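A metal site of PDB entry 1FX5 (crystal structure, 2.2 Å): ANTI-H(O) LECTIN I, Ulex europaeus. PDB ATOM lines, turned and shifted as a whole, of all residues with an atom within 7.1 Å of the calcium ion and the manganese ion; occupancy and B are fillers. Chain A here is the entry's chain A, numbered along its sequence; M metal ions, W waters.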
ATOM      1  N   ASP A  87       7.400  10.711 -20.696  1.00  0.00           N
ATOM      2  CA  ASP A  87       5.972  11.031 -20.876  1.00  0.00           C
ATOM      3  C   ASP A  87       5.783  12.228 -21.799  1.00  0.00           C
ATOM      4  O   ASP A  87       4.672  12.441 -22.295  1.00  0.00           O
ATOM      5  CB  ASP A  87       5.283  11.330 -19.550  1.00  0.00           C
ATOM      6  CG  ASP A  87       4.719  10.108 -18.908  1.00  0.00           C
ATOM      7  OD1 ASP A  87       5.394   9.565 -18.008  1.00  0.00           O
ATOM      8  OD2 ASP A  87       3.636   9.652 -19.322  1.00  0.00           O
ATOM      9  N   GLY A 104       4.879  12.067 -14.083  1.00  0.00           N
ATOM     10  CA  GLY A 104       4.423  10.938 -14.872  1.00  0.00           C
ATOM     11  C   GLY A 104       3.520  11.479 -15.976  1.00  0.00           C
ATOM     12  O   GLY A 104       3.776  12.568 -16.484  1.00  0.00           O
ATOM     13  N   GLY A 105       2.416  10.790 -16.303  1.00  0.00           N
ATOM     14  CA  GLY A 105       1.543  11.278 -17.358  1.00  0.00           C
ATOM     15  C   GLY A 105       0.733  12.543 -17.069  1.00  0.00           C
ATOM     16  O   GLY A 105      -0.060  12.991 -17.897  1.00  0.00           O
ATOM     17  N   TYR A 106       0.925  13.128 -15.902  1.00  0.00           N
ATOM     18  CA  TYR A 106       0.210  14.332 -15.524  1.00  0.00           C
ATOM     19  C   TYR A 106       1.092  15.581 -15.685  1.00  0.00           C
ATOM     20  O   TYR A 106       0.682  16.696 -15.301  1.00  0.00           O
ATOM     21  CB  TYR A 106      -0.394  14.178 -14.126  1.00  0.00           C
ATOM     22  CG  TYR A 106      -1.424  13.068 -14.054  1.00  0.00           C
ATOM     23  CD1 TYR A 106      -1.122  11.852 -13.459  1.00  0.00           C
ATOM     24  CD2 TYR A 106      -2.685  13.232 -14.586  1.00  0.00           C
ATOM     25  CE1 TYR A 106      -2.069  10.829 -13.392  1.00  0.00           C
ATOM     26  CE2 TYR A 106      -3.644  12.213 -14.531  1.00  0.00           C
ATOM     27  CZ  TYR A 106      -3.322  11.021 -13.933  1.00  0.00           C
ATOM     28  OH  TYR A 106      -4.277  10.031 -13.832  1.00  0.00           O
ATOM     29  N   PHE A 107       2.320  15.386 -16.188  1.00  0.00           N
ATOM     30  CA  PHE A 107       3.315  16.440 -16.441  1.00  0.00           C
ATOM     31  C   PHE A 107       3.685  17.438 -15.360  1.00  0.00           C
ATOM     32  O   PHE A 107       4.282  18.494 -15.681  1.00  0.00           O
ATOM     33  CB  PHE A 107       2.873  17.286 -17.659  1.00  0.00           C
ATOM     34  CG  PHE A 107       2.602  16.488 -18.894  1.00  0.00           C
ATOM     35  CD1 PHE A 107       1.293  16.290 -19.351  1.00  0.00           C
ATOM     36  CD2 PHE A 107       3.643  15.931 -19.620  1.00  0.00           C
ATOM     37  CE1 PHE A 107       1.031  15.550 -20.495  1.00  0.00           C
ATOM     38  CE2 PHE A 107       3.383  15.177 -20.769  1.00  0.00           C
ATOM     39  CZ  PHE A 107       2.075  14.991 -21.199  1.00  0.00           C
ATOM     40  N   GLU A 125       0.944  20.536 -25.094  1.00  0.00           N
ATOM     41  CA  GLU A 125       1.674  19.311 -24.780  1.00  0.00           C
ATOM     42  C   GLU A 125       2.226  18.517 -25.992  1.00  0.00           C
ATOM     43  O   GLU A 125       1.602  18.434 -27.050  1.00  0.00           O
ATOM     44  CB  GLU A 125       0.815  18.366 -23.901  1.00  0.00           C
ATOM     45  CG  GLU A 125      -0.430  17.836 -24.624  1.00  0.00           C
ATOM     46  CD  GLU A 125      -1.180  16.761 -23.867  1.00  0.00           C
ATOM     47  OE1 GLU A 125      -1.601  15.772 -24.495  1.00  0.00           O
ATOM     48  OE2 GLU A 125      -1.380  16.884 -22.649  1.00  0.00           O
ATOM     49  N   PHE A 126       3.407  17.932 -25.776  1.00  0.00           N
ATOM     50  CA  PHE A 126       4.169  17.104 -26.715  1.00  0.00           C
ATOM     51  C   PHE A 126       4.167  15.804 -25.900  1.00  0.00           C
ATOM     52  O   PHE A 126       5.117  15.500 -25.139  1.00  0.00           O
ATOM     53  CB  PHE A 126       5.576  17.692 -26.902  1.00  0.00           C
ATOM     54  CG  PHE A 126       5.564  19.103 -27.478  1.00  0.00           C
ATOM     55  CD1 PHE A 126       5.614  20.200 -26.630  1.00  0.00           C
ATOM     56  CD2 PHE A 126       5.433  19.322 -28.854  1.00  0.00           C
ATOM     57  CE1 PHE A 126       5.519  21.481 -27.152  1.00  0.00           C
ATOM     58  CE2 PHE A 126       5.350  20.617 -29.369  1.00  0.00           C
ATOM     59  CZ  PHE A 126       5.386  21.697 -28.519  1.00  0.00           C
ATOM     60  N   ASP A 127       3.035  15.116 -26.002  1.00  0.00           N
ATOM     61  CA  ASP A 127       2.746  13.873 -25.321  1.00  0.00           C
ATOM     62  C   ASP A 127       3.280  12.638 -26.028  1.00  0.00           C
ATOM     63  O   ASP A 127       2.739  12.220 -27.066  1.00  0.00           O
ATOM     64  CB  ASP A 127       1.222  13.830 -25.141  1.00  0.00           C
ATOM     65  CG  ASP A 127       0.778  12.808 -24.113  1.00  0.00           C
ATOM     66  OD1 ASP A 127      -0.355  12.923 -23.593  1.00  0.00           O
ATOM     67  OD2 ASP A 127       1.536  11.878 -23.826  1.00  0.00           O
ATOM     68  N   THR A 128       4.271  11.993 -25.399  1.00  0.00           N
ATOM     69  CA  THR A 128       4.880  10.794 -25.979  1.00  0.00           C
ATOM     70  C   THR A 128       4.203   9.437 -25.773  1.00  0.00           C
ATOM     71  O   THR A 128       4.694   8.434 -26.304  1.00  0.00           O
ATOM     72  CB  THR A 128       6.389  10.699 -25.629  1.00  0.00           C
ATOM     73  OG1 THR A 128       6.531  10.549 -24.212  1.00  0.00           O
ATOM     74  CG2 THR A 128       7.137  11.950 -26.074  1.00  0.00           C
ATOM     75  N   ILE A 129       3.121   9.373 -24.989  1.00  0.00           N
ATOM     76  CA  ILE A 129       2.408   8.097 -24.767  1.00  0.00           C
ATOM     77  C   ILE A 129       0.893   8.301 -24.571  1.00  0.00           C
ATOM     78  O   ILE A 129       0.471   9.140 -23.755  1.00  0.00           O
ATOM     79  CB  ILE A 129       3.018   7.287 -23.571  1.00  0.00           C
ATOM     80  CG1 ILE A 129       2.611   5.810 -23.662  1.00  0.00           C
ATOM     81  CG2 ILE A 129       2.605   7.872 -22.212  1.00  0.00           C
ATOM     82  CD1 ILE A 129       3.492   4.954 -24.613  1.00  0.00           C
ATOM     83  N   GLY A 130       0.092   7.540 -25.334  1.00  0.00           N
ATOM     84  CA  GLY A 130      -1.376   7.617 -25.248  1.00  0.00           C
ATOM     85  C   GLY A 130      -2.091   6.383 -24.681  1.00  0.00           C
ATOM     86  O   GLY A 130      -1.513   5.657 -23.872  1.00  0.00           O
ATOM     87  N   SER A 131      -3.348   6.138 -25.061  1.00  0.00           N
ATOM     88  CA  SER A 131      -4.049   4.963 -24.544  1.00  0.00           C
ATOM     89  C   SER A 131      -3.465   3.715 -25.203  1.00  0.00           C
ATOM     90  O   SER A 131      -3.000   3.777 -26.345  1.00  0.00           O
ATOM     91  CB  SER A 131      -5.553   5.045 -24.801  1.00  0.00           C
ATOM     92  OG  SER A 131      -5.803   5.291 -26.164  1.00  0.00           O
ATOM     93  N   VAL A 133      -2.131   2.954 -22.137  1.00  0.00           N
ATOM     94  CA  VAL A 133      -1.331   3.397 -20.989  1.00  0.00           C
ATOM     95  C   VAL A 133      -1.944   4.598 -20.277  1.00  0.00           C
ATOM     96  O   VAL A 133      -1.933   4.662 -19.058  1.00  0.00           O
ATOM     97  CB  VAL A 133       0.124   3.672 -21.394  1.00  0.00           C
ATOM     98  CG1 VAL A 133       0.935   4.100 -20.184  1.00  0.00           C
ATOM     99  CG2 VAL A 133       0.729   2.410 -22.011  1.00  0.00           C
ATOM    100  N   ASN A 134      -2.417   5.575 -21.054  1.00  0.00           N
ATOM    101  CA  ASN A 134      -3.050   6.767 -20.503  1.00  0.00           C
ATOM    102  C   ASN A 134      -4.440   6.677 -21.127  1.00  0.00           C
ATOM    103  O   ASN A 134      -4.617   7.024 -22.295  1.00  0.00           O
ATOM    104  CB  ASN A 134      -2.346   8.034 -20.982  1.00  0.00           C
ATOM    105  CG  ASN A 134      -1.034   8.293 -20.247  1.00  0.00           C
ATOM    106  OD1 ASN A 134      -0.267   9.195 -20.591  1.00  0.00           O
ATOM    107  ND2 ASN A 134      -0.767   7.495 -19.226  1.00  0.00           N
ATOM    108  N   TRP A 136      -7.062   8.469 -20.977  1.00  0.00           N
ATOM    109  CA  TRP A 136      -7.706   9.713 -21.412  1.00  0.00           C
ATOM    110  C   TRP A 136      -7.201  10.306 -22.735  1.00  0.00           C
ATOM    111  O   TRP A 136      -7.722  11.320 -23.188  1.00  0.00           O
ATOM    112  CB  TRP A 136      -7.505  10.772 -20.324  1.00  0.00           C
ATOM    113  CG  TRP A 136      -6.053  10.933 -19.923  1.00  0.00           C
ATOM    114  CD1 TRP A 136      -5.129  11.800 -20.483  1.00  0.00           C
ATOM    115  CD2 TRP A 136      -5.368  10.216 -18.884  1.00  0.00           C
ATOM    116  NE1 TRP A 136      -3.918  11.650 -19.845  1.00  0.00           N
ATOM    117  CE2 TRP A 136      -4.041  10.696 -18.855  1.00  0.00           C
ATOM    118  CE3 TRP A 136      -5.747   9.218 -17.978  1.00  0.00           C
ATOM    119  CZ2 TRP A 136      -3.095  10.213 -17.950  1.00  0.00           C
ATOM    120  CZ3 TRP A 136      -4.802   8.735 -17.072  1.00  0.00           C
ATOM    121  CH2 TRP A 136      -3.499   9.239 -17.071  1.00  0.00           C
ATOM    122  N   ASP A 137      -6.125   9.729 -23.300  1.00  0.00           N
ATOM    123  CA  ASP A 137      -5.503  10.166 -24.557  1.00  0.00           C
ATOM    124  C   ASP A 137      -5.928   9.408 -25.823  1.00  0.00           C
ATOM    125  O   ASP A 137      -6.562   8.351 -25.727  1.00  0.00           O
ATOM    126  CB  ASP A 137      -3.985   9.913 -24.487  1.00  0.00           C
ATOM    127  CG  ASP A 137      -3.236  10.916 -23.656  1.00  0.00           C
ATOM    128  OD1 ASP A 137      -2.225  10.472 -23.030  1.00  0.00           O
ATOM    129  OD2 ASP A 137      -3.601  12.112 -23.647  1.00  0.00           O
ATOM    130  N   PRO A 138      -5.608   9.945 -27.036  1.00  0.00           N
ATOM    131  CA  PRO A 138      -5.950   9.217 -28.254  1.00  0.00           C
ATOM    132  C   PRO A 138      -4.946   8.022 -28.252  1.00  0.00           C
ATOM    133  O   PRO A 138      -3.957   8.041 -27.506  1.00  0.00           O
ATOM    134  CB  PRO A 138      -5.646  10.228 -29.376  1.00  0.00           C
ATOM    135  CG  PRO A 138      -4.810  11.307 -28.718  1.00  0.00           C
ATOM    136  CD  PRO A 138      -5.334  11.365 -27.330  1.00  0.00           C
ATOM    137  N   PHE A 140      -2.182   7.051 -29.573  1.00  0.00           N
ATOM    138  CA  PHE A 140      -0.865   7.262 -30.191  1.00  0.00           C
ATOM    139  C   PHE A 140      -0.227   8.556 -29.676  1.00  0.00           C
ATOM    140  O   PHE A 140      -0.915   9.362 -29.050  1.00  0.00           O
ATOM    141  CB  PHE A 140      -0.997   7.366 -31.724  1.00  0.00           C
ATOM    142  CG  PHE A 140      -2.249   8.076 -32.206  1.00  0.00           C
ATOM    143  CD1 PHE A 140      -3.285   7.362 -32.805  1.00  0.00           C
ATOM    144  CD2 PHE A 140      -2.391   9.453 -32.042  1.00  0.00           C
ATOM    145  CE1 PHE A 140      -4.438   8.005 -33.221  1.00  0.00           C
ATOM    146  CE2 PHE A 140      -3.552  10.102 -32.457  1.00  0.00           C
ATOM    147  CZ  PHE A 140      -4.574   9.372 -33.050  1.00  0.00           C
ATOM    148  N   HIS A 142       1.074  12.336 -29.490  1.00  0.00           N
ATOM    149  CA  HIS A 142       0.377  13.470 -30.109  1.00  0.00           C
ATOM    150  C   HIS A 142       0.714  14.823 -29.502  1.00  0.00           C
ATOM    151  O   HIS A 142       1.336  14.886 -28.430  1.00  0.00           O
ATOM    152  CB  HIS A 142      -1.126  13.232 -29.873  1.00  0.00           C
ATOM    153  CG  HIS A 142      -1.470  12.986 -28.414  1.00  0.00           C
ATOM    154  ND1 HIS A 142      -1.212  11.798 -27.749  1.00  0.00           N
ATOM    155  CD2 HIS A 142      -1.993  13.824 -27.485  1.00  0.00           C
ATOM    156  CE1 HIS A 142      -1.563  11.945 -26.460  1.00  0.00           C
ATOM    157  NE2 HIS A 142      -2.055  13.152 -26.239  1.00  0.00           N
ATOM    158  N   ILE A 143       0.429  15.911 -30.233  1.00  0.00           N
ATOM    159  CA  ILE A 143       0.696  17.235 -29.671  1.00  0.00           C
ATOM    160  C   ILE A 143      -0.725  17.807 -29.452  1.00  0.00           C
ATOM    161  O   ILE A 143      -1.589  17.716 -30.347  1.00  0.00           O
ATOM    162  CB  ILE A 143       1.638  18.209 -30.502  1.00  0.00           C
ATOM    163  CG1 ILE A 143       0.871  19.045 -31.517  1.00  0.00           C
ATOM    164  CG2 ILE A 143       2.777  17.449 -31.130  1.00  0.00           C
ATOM    165  CD1 ILE A 143       0.383  18.279 -32.721  1.00  0.00           C
ATOM    166  N   GLY A 144      -1.007  18.276 -28.227  1.00  0.00           N
ATOM    167  CA  GLY A 144      -2.328  18.818 -27.959  1.00  0.00           C
ATOM    168  C   GLY A 144      -2.424  20.092 -27.141  1.00  0.00           C
ATOM    169  O   GLY A 144      -1.436  20.595 -26.582  1.00  0.00           O
ATOM    170  N   ASP A 146      -4.242  21.801 -23.948  1.00  0.00           N
ATOM    171  CA  ASP A 146      -4.938  21.543 -22.685  1.00  0.00           C
ATOM    172  C   ASP A 146      -5.430  22.805 -22.015  1.00  0.00           C
ATOM    173  O   ASP A 146      -4.671  23.756 -21.837  1.00  0.00           O
ATOM    174  CB  ASP A 146      -4.015  20.839 -21.687  1.00  0.00           C
ATOM    175  CG  ASP A 146      -3.417  19.552 -22.218  1.00  0.00           C
ATOM    176  OD1 ASP A 146      -3.868  19.022 -23.254  1.00  0.00           O
ATOM    177  OD2 ASP A 146      -2.490  19.054 -21.596  1.00  0.00           O
ATOM    178  N   VAL A 150      -6.008  17.510 -17.983  1.00  0.00           N
ATOM    179  CA  VAL A 150      -4.996  16.678 -18.640  1.00  0.00           C
ATOM    180  C   VAL A 150      -5.576  16.129 -19.979  1.00  0.00           C
ATOM    181  O   VAL A 150      -4.846  15.609 -20.820  1.00  0.00           O
ATOM    182  CB  VAL A 150      -4.481  15.515 -17.703  1.00  0.00           C
ATOM    183  CG1 VAL A 150      -5.557  14.435 -17.506  1.00  0.00           C
ATOM    184  CG2 VAL A 150      -3.181  14.908 -18.263  1.00  0.00           C
ATOM    185  N   LYS A 151      -6.891  16.230 -20.130  1.00  0.00           N
ATOM    186  CA  LYS A 151      -7.554  15.763 -21.352  1.00  0.00           C
ATOM    187  C   LYS A 151      -7.607  16.974 -22.311  1.00  0.00           C
ATOM    188  O   LYS A 151      -8.070  18.036 -21.904  1.00  0.00           O
ATOM    189  CB  LYS A 151      -8.970  15.296 -21.030  1.00  0.00           C
ATOM    190  CG  LYS A 151      -9.692  14.684 -22.211  1.00  0.00           C
ATOM    191  CD  LYS A 151     -11.051  14.200 -21.766  1.00  0.00           C
ATOM    192  CE  LYS A 151     -11.726  13.369 -22.842  1.00  0.00           C
ATOM    193  NZ  LYS A 151     -10.987  12.114 -23.139  1.00  0.00           N
ATOM    194  N   SER A 152      -7.103  16.826 -23.531  1.00  0.00           N
ATOM    195  CA  SER A 152      -7.088  17.918 -24.516  1.00  0.00           C
ATOM    196  C   SER A 152      -8.418  18.255 -25.219  1.00  0.00           C
ATOM    197  O   SER A 152      -9.290  17.380 -25.352  1.00  0.00           O
ATOM    198  CB  SER A 152      -6.091  17.575 -25.633  1.00  0.00           C
ATOM    199  OG  SER A 152      -4.817  17.163 -25.146  1.00  0.00           O
ATOM    200  N   ALA A 155      -6.232  17.691 -30.474  1.00  0.00           N
ATOM    201  CA  ALA A 155      -4.924  17.028 -30.531  1.00  0.00           C
ATOM    202  C   ALA A 155      -4.633  16.495 -31.944  1.00  0.00           C
ATOM    203  O   ALA A 155      -5.574  16.215 -32.689  1.00  0.00           O
ATOM    204  CB  ALA A 155      -4.901  15.854 -29.539  1.00  0.00           C
HETATM  205 CA    CA M   1       0.014  10.824 -22.154  1.00  0.00          CA
HETATM  206 MN    MN M   2      -2.309  13.772 -23.975  1.00  0.00          MN
HETATM  207  O   HOH W   1       2.117  11.085 -21.262  1.00  0.00           O
HETATM  208  O   HOH W   2      -2.570  14.522 -22.010  1.00  0.00           O
HETATM  209  O   HOH W   3      -0.825  12.408 -20.647  1.00  0.00           O
HETATM  210  O   HOH W   4      -4.234  14.585 -24.652  1.00  0.00           O
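The manganese ion is bound by water W2, 2.1 Å away. OD2 of Asp 137 binds the manganese ion. OD1 of Asp 127 binds the manganese ion (2.2 Å). The manganese ion is bound by the side-chain carboxylate (OE1) of Glu 125 (2.2 Å). The manganese ion is bound by water W4 (2.2 Å). NE2 of His 142 is bound to the manganese ion, 2.4 Å away. The manganese ion has six donor atoms within binding distance.
The side-chain amide oxygen (OD1) of Asn 134 is bound to the calcium ion (2.3 Å). The calcium ion is bound by water W1, 2.3 Å away. Water W3 binds the calcium ion, at 2.3 Å. O of Ile 129 is bound to the calcium ion, 2.4 Å away. The calcium ion is bound by the side-chain carboxylate (OD1) of Asp 137 (2.4 Å). OD2 of Asp 127 binds the calcium ion (2.5 Å). The calcium ion is bound by the side-chain carboxylate (OD1) of Asp 127, 2.6 Å away. The calcium ion has seven donor atoms within binding distance.
Of the 26 residues printed, 4 come within 4 Å of the manganese ion. The nearest printed residue that does not touch the manganese ion is Ser 152 (4.4 Å).
The nearest printed residue that does not touch the calcium ion is Gly 130 (4.6 Å).
Water W3 bridges O of Gly 105 (2.9 Å) and NE1 of Trp 136 (3.3 Å). Water W2 lies within hydrogen-bond range of the side-chain carboxylate of Glu 125 (2.7 Å) and the backbone carbonyl oxygen of Val 150 (2.8 Å).
ND1 of His 142 is in hydrogen-bond range of O of Phe 140 (2.8 Å). The backbone carbonyl oxygen (O) of Asp 137 lies within hydrogen-bond range of the side-chain hydroxyl (OG) of Ser 131, at 3.2 Å. The side-chain carboxylate of Asp 146 sits close to the side-chain carboxylate of Glu 125 (2.7 Å). N of Glu 125 is in hydrogen-bond range of O of Gly 144, at 2.8 Å.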
